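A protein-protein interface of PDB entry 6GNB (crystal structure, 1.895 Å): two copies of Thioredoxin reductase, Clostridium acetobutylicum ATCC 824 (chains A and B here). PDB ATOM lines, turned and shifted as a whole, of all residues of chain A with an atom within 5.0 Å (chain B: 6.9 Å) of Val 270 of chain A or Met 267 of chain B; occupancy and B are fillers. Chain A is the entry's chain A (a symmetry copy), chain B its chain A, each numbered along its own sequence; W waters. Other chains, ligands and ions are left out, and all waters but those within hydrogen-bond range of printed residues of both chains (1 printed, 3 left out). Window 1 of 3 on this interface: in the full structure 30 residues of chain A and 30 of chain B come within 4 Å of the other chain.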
ATOM      1  N   PRO A  16      17.944 -25.633  11.278  1.00  0.00           N
ATOM      2  CA  PRO A  16      18.170 -25.606  12.728  1.00  0.00           C
ATOM      3  C   PRO A  16      16.895 -25.598  13.560  1.00  0.00           C
ATOM      4  O   PRO A  16      16.766 -26.362  14.524  1.00  0.00           O
ATOM      5  CB  PRO A  16      19.001 -24.327  12.908  1.00  0.00           C
ATOM      6  CG  PRO A  16      19.762 -24.212  11.607  1.00  0.00           C
ATOM      7  CD  PRO A  16      18.869 -24.767  10.537  1.00  0.00           C
ATOM      8  N   ALA A  17      15.943 -24.709  13.248  1.00  0.00           N
ATOM      9  CA  ALA A  17      14.720 -24.616  14.042  1.00  0.00           C
ATOM     10  C   ALA A  17      13.899 -25.905  13.964  1.00  0.00           C
ATOM     11  O   ALA A  17      13.446 -26.434  14.988  1.00  0.00           O
ATOM     12  CB  ALA A  17      13.897 -23.393  13.623  1.00  0.00           C
ATOM     13  N   ALA A  20      15.642 -28.800  15.743  1.00  0.00           N
ATOM     14  CA  ALA A  20      15.534 -28.622  17.184  1.00  0.00           C
ATOM     15  C   ALA A  20      14.144 -29.009  17.665  1.00  0.00           C
ATOM     16  O   ALA A  20      13.993 -29.641  18.714  1.00  0.00           O
ATOM     17  CB  ALA A  20      15.859 -27.175  17.551  1.00  0.00           C
ATOM     18  N   ILE A  23      13.920 -33.088  17.566  1.00  0.00           N
ATOM     19  CA  ILE A  23      14.595 -33.869  18.605  1.00  0.00           C
ATOM     20  C   ILE A  23      13.924 -33.692  19.960  1.00  0.00           C
ATOM     21  O   ILE A  23      14.100 -34.535  20.849  1.00  0.00           O
ATOM     22  CB  ILE A  23      16.103 -33.582  18.678  1.00  0.00           C
ATOM     23  CG1 ILE A  23      16.399 -32.162  19.158  1.00  0.00           C
ATOM     24  CG2 ILE A  23      16.760 -33.836  17.332  1.00  0.00           C
ATOM     25  CD1 ILE A  23      17.886 -31.922  19.417  1.00  0.00           C
ATOM     26  N   ASN A  24      13.174 -32.612  20.144  1.00  0.00           N
ATOM     27  CA  ASN A  24      12.444 -32.396  21.386  1.00  0.00           C
ATOM     28  C   ASN A  24      11.040 -32.969  21.351  1.00  0.00           C
ATOM     29  O   ASN A  24      10.469 -33.243  22.409  1.00  0.00           O
ATOM     30  CB  ASN A  24      12.401 -30.903  21.715  1.00  0.00           C
ATOM     31  CG  ASN A  24      13.690 -30.424  22.309  1.00  0.00           C
ATOM     32  OD1 ASN A  24      13.920 -30.599  23.519  1.00  0.00           O
ATOM     33  ND2 ASN A  24      14.570 -29.867  21.474  1.00  0.00           N
ATOM     34  N   TYR A  53      28.048 -20.490  17.817  1.00  0.00           N
ATOM     35  CA  TYR A  53      27.238 -21.629  18.227  1.00  0.00           C
ATOM     36  C   TYR A  53      27.983 -22.325  19.364  1.00  0.00           C
ATOM     37  O   TYR A  53      28.985 -23.016  19.136  1.00  0.00           O
ATOM     38  CB  TYR A  53      26.950 -22.552  17.049  1.00  0.00           C
ATOM     39  CG  TYR A  53      25.875 -23.572  17.336  1.00  0.00           C
ATOM     40  CD1 TYR A  53      24.557 -23.279  17.142  1.00  0.00           C
ATOM     41  CD2 TYR A  53      26.204 -24.864  17.738  1.00  0.00           C
ATOM     42  CE1 TYR A  53      23.563 -24.208  17.402  1.00  0.00           C
ATOM     43  CE2 TYR A  53      25.212 -25.820  18.007  1.00  0.00           C
ATOM     44  CZ  TYR A  53      23.872 -25.463  17.825  1.00  0.00           C
ATOM     45  OH  TYR A  53      22.783 -26.296  18.044  1.00  0.00           O
ATOM     46  N   TYR A 266      21.652 -19.112  14.554  1.00  0.00           N
ATOM     47  CA  TYR A 266      21.408 -20.513  14.899  1.00  0.00           C
ATOM     48  C   TYR A 266      20.909 -20.790  16.321  1.00  0.00           C
ATOM     49  O   TYR A 266      19.966 -21.557  16.499  1.00  0.00           O
ATOM     50  CB  TYR A 266      22.695 -21.329  14.721  1.00  0.00           C
ATOM     51  CG  TYR A 266      23.294 -21.303  13.335  1.00  0.00           C
ATOM     52  CD1 TYR A 266      22.592 -21.791  12.242  1.00  0.00           C
ATOM     53  CD2 TYR A 266      24.578 -20.820  13.127  1.00  0.00           C
ATOM     54  CE1 TYR A 266      23.146 -21.777  10.976  1.00  0.00           C
ATOM     55  CE2 TYR A 266      25.139 -20.803  11.866  1.00  0.00           C
ATOM     56  CZ  TYR A 266      24.421 -21.281  10.795  1.00  0.00           C
ATOM     57  OH  TYR A 266      24.979 -21.264   9.539  1.00  0.00           O
ATOM     58  N   MET A 267      21.520 -20.173  17.330  1.00  0.00           N
ATOM     59  CA  MET A 267      21.111 -20.440  18.712  1.00  0.00           C
ATOM     60  C   MET A 267      19.681 -19.978  18.978  1.00  0.00           C
ATOM     61  O   MET A 267      18.902 -20.696  19.603  1.00  0.00           O
ATOM     62  CB  MET A 267      22.123 -19.871  19.706  1.00  0.00           C
ATOM     63  CG  MET A 267      23.473 -20.566  19.584  1.00  0.00           C
ATOM     64  SD  MET A 267      24.467 -20.590  21.087  1.00  0.00           S
ATOM     65  CE  MET A 267      24.748 -18.836  21.318  1.00  0.00           C
ATOM     66  N   LYS A 268      19.330 -18.791  18.498  1.00  0.00           N
ATOM     67  CA  LYS A 268      17.947 -18.339  18.598  1.00  0.00           C
ATOM     68  C   LYS A 268      17.016 -19.359  17.956  1.00  0.00           C
ATOM     69  O   LYS A 268      16.010 -19.764  18.547  1.00  0.00           O
ATOM     70  CB  LYS A 268      17.775 -16.975  17.935  1.00  0.00           C
ATOM     71  CG  LYS A 268      16.297 -16.533  17.913  1.00  0.00           C
ATOM     72  CD  LYS A 268      16.013 -15.196  17.245  1.00  0.00           C
ATOM     73  CE  LYS A 268      15.516 -15.314  15.789  1.00  0.00           C
ATOM     74  NZ  LYS A 268      14.181 -15.930  15.480  1.00  0.00           N
ATOM     75  N   ALA A 269      17.364 -19.820  16.754  1.00  0.00           N
ATOM     76  CA  ALA A 269      16.500 -20.755  16.047  1.00  0.00           C
ATOM     77  C   ALA A 269      16.315 -22.062  16.809  1.00  0.00           C
ATOM     78  O   ALA A 269      15.196 -22.572  16.914  1.00  0.00           O
ATOM     79  CB  ALA A 269      17.068 -21.017  14.649  1.00  0.00           C
ATOM     80  N   VAL A 270      17.399 -22.653  17.329  1.00  0.00           N
ATOM     81  CA  VAL A 270      17.234 -23.946  17.995  1.00  0.00           C
ATOM     82  C   VAL A 270      16.482 -23.792  19.304  1.00  0.00           C
ATOM     83  O   VAL A 270      15.701 -24.668  19.704  1.00  0.00           O
ATOM     84  CB  VAL A 270      18.568 -24.713  18.144  1.00  0.00           C
ATOM     85  CG1 VAL A 270      19.171 -24.998  16.783  1.00  0.00           C
ATOM     86  CG2 VAL A 270      19.599 -23.999  19.020  1.00  0.00           C
ATOM     87  N   GLY A 271      16.713 -22.688  19.998  1.00  0.00           N
ATOM     88  CA  GLY A 271      15.944 -22.425  21.209  1.00  0.00           C
ATOM     89  C   GLY A 271      14.453 -22.305  20.944  1.00  0.00           C
ATOM     90  O   GLY A 271      13.627 -22.868  21.665  1.00  0.00           O
ATOM     91  N   GLU A 272      14.097 -21.539  19.925  1.00  0.00           N
ATOM     92  CA  GLU A 272      12.691 -21.414  19.537  1.00  0.00           C
ATOM     93  C   GLU A 272      12.095 -22.753  19.104  1.00  0.00           C
ATOM     94  O   GLU A 272      10.952 -23.079  19.449  1.00  0.00           O
ATOM     95  CB  GLU A 272      12.560 -20.376  18.420  1.00  0.00           C
ATOM     96  CG  GLU A 272      12.814 -18.965  18.925  1.00  0.00           C
ATOM     97  CD  GLU A 272      12.547 -17.877  17.914  1.00  0.00           C
ATOM     98  OE1 GLU A 272      12.266 -18.148  16.728  1.00  0.00           O
ATOM     99  OE2 GLU A 272      12.593 -16.697  18.320  1.00  0.00           O
ATOM    100  N   GLY A 273      12.835 -23.546  18.335  1.00  0.00           N
ATOM    101  CA  GLY A 273      12.301 -24.847  17.953  1.00  0.00           C
ATOM    102  C   GLY A 273      12.026 -25.722  19.163  1.00  0.00           C
ATOM    103  O   GLY A 273      10.995 -26.408  19.232  1.00  0.00           O
ATOM    104  N   GLN A 274      12.933 -25.703  20.134  1.00  0.00           N
ATOM    105  CA  GLN A 274      12.727 -26.475  21.347  1.00  0.00           C
ATOM    106  C   GLN A 274      11.477 -26.028  22.088  1.00  0.00           C
ATOM    107  O   GLN A 274      10.664 -26.855  22.509  1.00  0.00           O
ATOM    108  CB  GLN A 274      13.946 -26.330  22.249  1.00  0.00           C
ATOM    109  CG  GLN A 274      13.751 -26.963  23.572  1.00  0.00           C
ATOM    110  CD  GLN A 274      15.050 -27.090  24.285  1.00  0.00           C
ATOM    111  OE1 GLN A 274      15.694 -26.092  24.619  1.00  0.00           O
ATOM    112  NE2 GLN A 274      15.501 -28.336  24.462  1.00  0.00           N
ATOM    113  N   PRO B  16      24.911 -21.916  30.561  1.00  0.00           N
ATOM    114  CA  PRO B  16      24.568 -21.851  29.135  1.00  0.00           C
ATOM    115  C   PRO B  16      24.106 -20.479  28.665  1.00  0.00           C
ATOM    116  O   PRO B  16      24.566 -19.978  27.631  1.00  0.00           O
ATOM    117  CB  PRO B  16      23.471 -22.919  29.010  1.00  0.00           C
ATOM    118  CG  PRO B  16      23.833 -23.925  30.078  1.00  0.00           C
ATOM    119  CD  PRO B  16      24.452 -23.153  31.204  1.00  0.00           C
ATOM    120  N   ASN B  52      19.080 -33.757  23.709  1.00  0.00           N
ATOM    121  CA  ASN B  52      18.276 -32.703  23.110  1.00  0.00           C
ATOM    122  C   ASN B  52      19.054 -31.409  22.952  1.00  0.00           C
ATOM    123  O   ASN B  52      18.446 -30.332  22.921  1.00  0.00           O
ATOM    124  CB  ASN B  52      16.989 -32.489  23.906  1.00  0.00           C
ATOM    125  CG  ASN B  52      17.245 -31.900  25.269  1.00  0.00           C
ATOM    126  OD1 ASN B  52      18.381 -31.818  25.717  1.00  0.00           O
ATOM    127  ND2 ASN B  52      16.175 -31.444  25.926  1.00  0.00           N
ATOM    128  N   TYR B  53      20.369 -31.479  22.864  1.00  0.00           N
ATOM    129  CA  TYR B  53      21.190 -30.348  22.452  1.00  0.00           C
ATOM    130  C   TYR B  53      21.714 -30.659  21.051  1.00  0.00           C
ATOM    131  O   TYR B  53      22.620 -31.486  20.882  1.00  0.00           O
ATOM    132  CB  TYR B  53      22.303 -30.080  23.458  1.00  0.00           C
ATOM    133  CG  TYR B  53      22.990 -28.753  23.252  1.00  0.00           C
ATOM    134  CD1 TYR B  53      22.505 -27.612  23.822  1.00  0.00           C
ATOM    135  CD2 TYR B  53      24.181 -28.667  22.533  1.00  0.00           C
ATOM    136  CE1 TYR B  53      23.128 -26.389  23.638  1.00  0.00           C
ATOM    137  CE2 TYR B  53      24.828 -27.437  22.336  1.00  0.00           C
ATOM    138  CZ  TYR B  53      24.274 -26.290  22.912  1.00  0.00           C
ATOM    139  OH  TYR B  53      24.798 -25.008  22.811  1.00  0.00           O
ATOM    140  N   LEU B  54      21.154 -29.957  20.067  1.00  0.00           N
ATOM    141  CA  LEU B  54      21.299 -30.328  18.665  1.00  0.00           C
ATOM    142  C   LEU B  54      22.759 -30.254  18.233  1.00  0.00           C
ATOM    143  O   LEU B  54      23.421 -29.218  18.379  1.00  0.00           O
ATOM    144  CB  LEU B  54      20.440 -29.418  17.798  1.00  0.00           C
ATOM    145  CG  LEU B  54      20.410 -29.776  16.303  1.00  0.00           C
ATOM    146  CD1 LEU B  54      19.792 -31.152  16.029  1.00  0.00           C
ATOM    147  CD2 LEU B  54      19.690 -28.690  15.520  1.00  0.00           C
ATOM    148  N   GLY B  55      23.247 -31.351  17.674  1.00  0.00           N
ATOM    149  CA  GLY B  55      24.632 -31.488  17.284  1.00  0.00           C
ATOM    150  C   GLY B  55      25.506 -32.249  18.258  1.00  0.00           C
ATOM    151  O   GLY B  55      26.626 -32.631  17.884  1.00  0.00           O
ATOM    152  N   GLN B 265      15.589 -25.685  29.687  1.00  0.00           N
ATOM    153  CA  GLN B 265      16.393 -26.485  28.767  1.00  0.00           C
ATOM    154  C   GLN B 265      17.583 -25.687  28.238  1.00  0.00           C
ATOM    155  O   GLN B 265      17.548 -24.457  28.201  1.00  0.00           O
ATOM    156  CB  GLN B 265      15.546 -26.941  27.572  1.00  0.00           C
ATOM    157  CG  GLN B 265      14.337 -27.815  27.888  1.00  0.00           C
ATOM    158  CD  GLN B 265      14.703 -29.242  28.243  1.00  0.00           C
ATOM    159  OE1 GLN B 265      14.417 -30.169  27.488  1.00  0.00           O
ATOM    160  NE2 GLN B 265      15.342 -29.425  29.391  1.00  0.00           N
ATOM    161  N   TYR B 266      18.629 -26.392  27.821  1.00  0.00           N
ATOM    162  CA  TYR B 266      19.826 -25.748  27.277  1.00  0.00           C
ATOM    163  C   TYR B 266      19.638 -24.926  25.998  1.00  0.00           C
ATOM    164  O   TYR B 266      20.137 -23.807  25.912  1.00  0.00           O
ATOM    165  CB  TYR B 266      20.894 -26.803  26.965  1.00  0.00           C
ATOM    166  CG  TYR B 266      21.330 -27.652  28.135  1.00  0.00           C
ATOM    167  CD1 TYR B 266      21.929 -27.082  29.250  1.00  0.00           C
ATOM    168  CD2 TYR B 266      21.173 -29.030  28.109  1.00  0.00           C
ATOM    169  CE1 TYR B 266      22.338 -27.861  30.316  1.00  0.00           C
ATOM    170  CE2 TYR B 266      21.580 -29.816  29.168  1.00  0.00           C
ATOM    171  CZ  TYR B 266      22.160 -29.228  30.268  1.00  0.00           C
ATOM    172  OH  TYR B 266      22.565 -30.010  31.323  1.00  0.00           O
ATOM    173  N   MET B 267      18.920 -25.458  25.011  1.00  0.00           N
ATOM    174  CA  MET B 267      18.750 -24.731  23.750  1.00  0.00           C
ATOM    175  C   MET B 267      17.968 -23.435  23.944  1.00  0.00           C
ATOM    176  O   MET B 267      18.343 -22.395  23.403  1.00  0.00           O
ATOM    177  CB  MET B 267      18.160 -25.635  22.668  1.00  0.00           C
ATOM    178  CG  MET B 267      19.112 -26.769  22.310  1.00  0.00           C
ATOM    179  SD  MET B 267      18.955 -27.410  20.634  1.00  0.00           S
ATOM    180  CE  MET B 267      17.287 -28.063  20.691  1.00  0.00           C
ATOM    181  N   LYS B 268      16.893 -23.489  24.721  1.00  0.00           N
ATOM    182  CA  LYS B 268      16.170 -22.269  25.059  1.00  0.00           C
ATOM    183  C   LYS B 268      17.117 -21.261  25.698  1.00  0.00           C
ATOM    184  O   LYS B 268      17.158 -20.090  25.308  1.00  0.00           O
ATOM    185  CB  LYS B 268      15.007 -22.572  26.001  1.00  0.00           C
ATOM    186  CG  LYS B 268      14.306 -21.283  26.476  1.00  0.00           C
ATOM    187  CD  LYS B 268      13.148 -21.474  27.444  1.00  0.00           C
ATOM    188  CE  LYS B 268      13.526 -21.261  28.925  1.00  0.00           C
ATOM    189  NZ  LYS B 268      13.927 -19.904  29.428  1.00  0.00           N
ATOM    190  N   ALA B 269      17.920 -21.715  26.661  1.00  0.00           N
ATOM    191  CA  ALA B 269      18.815 -20.805  27.361  1.00  0.00           C
ATOM    192  C   ALA B 269      19.830 -20.157  26.426  1.00  0.00           C
ATOM    193  O   ALA B 269      20.070 -18.948  26.504  1.00  0.00           O
ATOM    194  CB  ALA B 269      19.522 -21.555  28.493  1.00  0.00           C
ATOM    195  N   VAL B 270      20.472 -20.938  25.547  1.00  0.00           N
ATOM    196  CA  VAL B 270      21.502 -20.331  24.702  1.00  0.00           C
ATOM    197  C   VAL B 270      20.884 -19.397  23.677  1.00  0.00           C
ATOM    198  O   VAL B 270      21.464 -18.361  23.319  1.00  0.00           O
ATOM    199  CB  VAL B 270      22.452 -21.378  24.077  1.00  0.00           C
ATOM    200  CG1 VAL B 270      23.178 -22.150  25.161  1.00  0.00           C
ATOM    201  CG2 VAL B 270      21.757 -22.359  23.131  1.00  0.00           C
ATOM    202  N   GLY B 271      19.709 -19.751  23.180  1.00  0.00           N
ATOM    203  CA  GLY B 271      19.008 -18.846  22.275  1.00  0.00           C
ATOM    204  C   GLY B 271      18.670 -17.514  22.920  1.00  0.00           C
ATOM    205  O   GLY B 271      18.865 -16.449  22.331  1.00  0.00           O
ATOM    206  N   GLU B 272      18.128 -17.566  24.126  1.00  0.00           N
ATOM    207  CA  GLU B 272      17.833 -16.339  24.868  1.00  0.00           C
ATOM    208  C   GLU B 272      19.095 -15.529  25.162  1.00  0.00           C
ATOM    209  O   GLU B 272      19.096 -14.296  25.055  1.00  0.00           O
ATOM    210  CB  GLU B 272      17.100 -16.691  26.165  1.00  0.00           C
ATOM    211  CG  GLU B 272      15.685 -17.179  25.901  1.00  0.00           C
ATOM    212  CD  GLU B 272      14.852 -17.393  27.142  1.00  0.00           C
ATOM    213  OE1 GLU B 272      15.349 -17.294  28.283  1.00  0.00           O
ATOM    214  OE2 GLU B 272      13.640 -17.648  26.978  1.00  0.00           O
ATOM    215  N   GLY B 273      20.182 -16.187  25.551  1.00  0.00           N
ATOM    216  CA  GLY B 273      21.408 -15.437  25.789  1.00  0.00           C
ATOM    217  C   GLY B 273      21.884 -14.721  24.537  1.00  0.00           C
ATOM    218  O   GLY B 273      22.317 -13.561  24.592  1.00  0.00           O
HETATM  219  O   HOH W   1      13.267 -32.905  25.240  1.00  0.00           O
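The side-chain amide oxygen (OD1) of Asn 24 of chain A is in hydrogen-bond range of the side-chain amide nitrogen (ND2) of Asn 52 of chain B, 3.4 Å away. The backbone carbonyl oxygen (O) of Leu 54 of chain B is in hydrogen-bond range of the side-chain hydroxyl (OH) of Tyr 53 of chain A, 3.0 Å away. N of Lys 268 of chain B lies within hydrogen-bond range of OE1 of Gln 274 of chain A (2.9 Å). OE1 of Gln 274 of chain A sits close to N of Met 267 of chain B (3.3 Å).
The side-chain amide nitrogen of Gln 274 of chain A sits at hydrogen-bond distance from the side-chain amide oxygen of Asn 24 of chain A (2.9 Å). OE1 of Gln 265 of chain B is in hydrogen-bond range of ND2 of Asn 52 of chain B (2.7 Å). NZ of Lys 268 of chain A lies within salt-bridge range of OE1 of Glu 272 of chain A. The side-chain amino group of Lys 268 of chain B lies within salt-bridge range of the side-chain carboxylate of Glu 272 of chain B (3.2 Å). The side-chain amide nitrogen (ND2) of Asn 24 of chain A sits at hydrogen-bond distance from the backbone carbonyl oxygen (O) of Ala 20 of chain A (2.8 Å). N of Leu 54 of chain B is in hydrogen-bond range of SD of Met 267 of chain B (3.4 Å).
Among the printed residues, pairs that only touch across the chains: Pro 16 of chain A with Leu 54 of chain B (3.9 Å), Ala 20 of chain A with Met 267 of chain B (3.6 Å), Ile 23 of chain A with Asn 52 of chain B (3.8 Å), Ile 23 of chain A with Leu 54 of chain B (3.8 Å), Asn 24 of chain A with Met 267 of chain B (3.4 Å), Met 267 of chain A with Val 270 of chain B (3.7 Å), Met 267 of chain A with Gly 271 of chain B (3.3 Å), Lys 268 of chain A with Gly 271 of chain B (3.8 Å), Val 270 of chain A with Leu 54 of chain B (3.9 Å), Val 270 of chain A with Met 267 of chain B (3.7 Å), Gly 271 of chain A with Met 267 of chain B (3.3 Å), Gly 271 of chain A with Lys 268 of chain B (3.8 Å), Gln 274 of chain A with Asn 52 of chain B (3.5 Å) and Gln 274 of chain A with Gln 265 of chain B (3.1 Å).
Of chain B, only Leu 54 and Met 267 come within 4 Å of Val 270 of chain A. Met 267 of chain B touches just these residues of chain A: Ala 20 (3.6 Å), Asn 24 (3.4 Å), Val 270 (3.7 Å), Gly 271 (3.3 Å) and Gln 274 (3.2 Å). Printed residues of chain B within 4 Å of Lys 268 of chain A: Gly 271. Of the printed residues of chain B, Ile 23 of chain A touches Asn 52 and Leu 54. The nearest residue of chain B that does not touch Val 270 of chain A is Val 270 of chain B (4.9 Å). The nearest residue of chain A that does not touch Met 267 of chain B is Ile 23 of chain A (4.1 Å). The nearest printed residue of chain A that does not touch Leu 54 of chain B is Ala 20 of chain A (4.1 Å).
Among the printed residues, 18 pairs touch across the chains.
Met 267 of chain A touches Val 270 of chain B, and with the chains exchanged Val 270 of chain A touches Met 267 of chain B. Met 267 of chain A touches Gly 271 of chain B, and with the chains exchanged Gly 271 of chain A touches Met 267 of chain B. Lys 268 of chain A touches Gly 271 of chain B, and with the chains exchanged Gly 271 of chain A touches Lys 268 of chain B. Positions printed for both chains: 16, 53, 266, 267, 268, 269, 270, 271, 272 and 273. Of the 18 pairs that touch across the chains among the printed residues, 6 have their exchanged pair printed and touching as well.
Water W1 lies within hydrogen-bond range of OD1 of Asn 24 of chain A and ND2 of Asn 52 of chain B.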
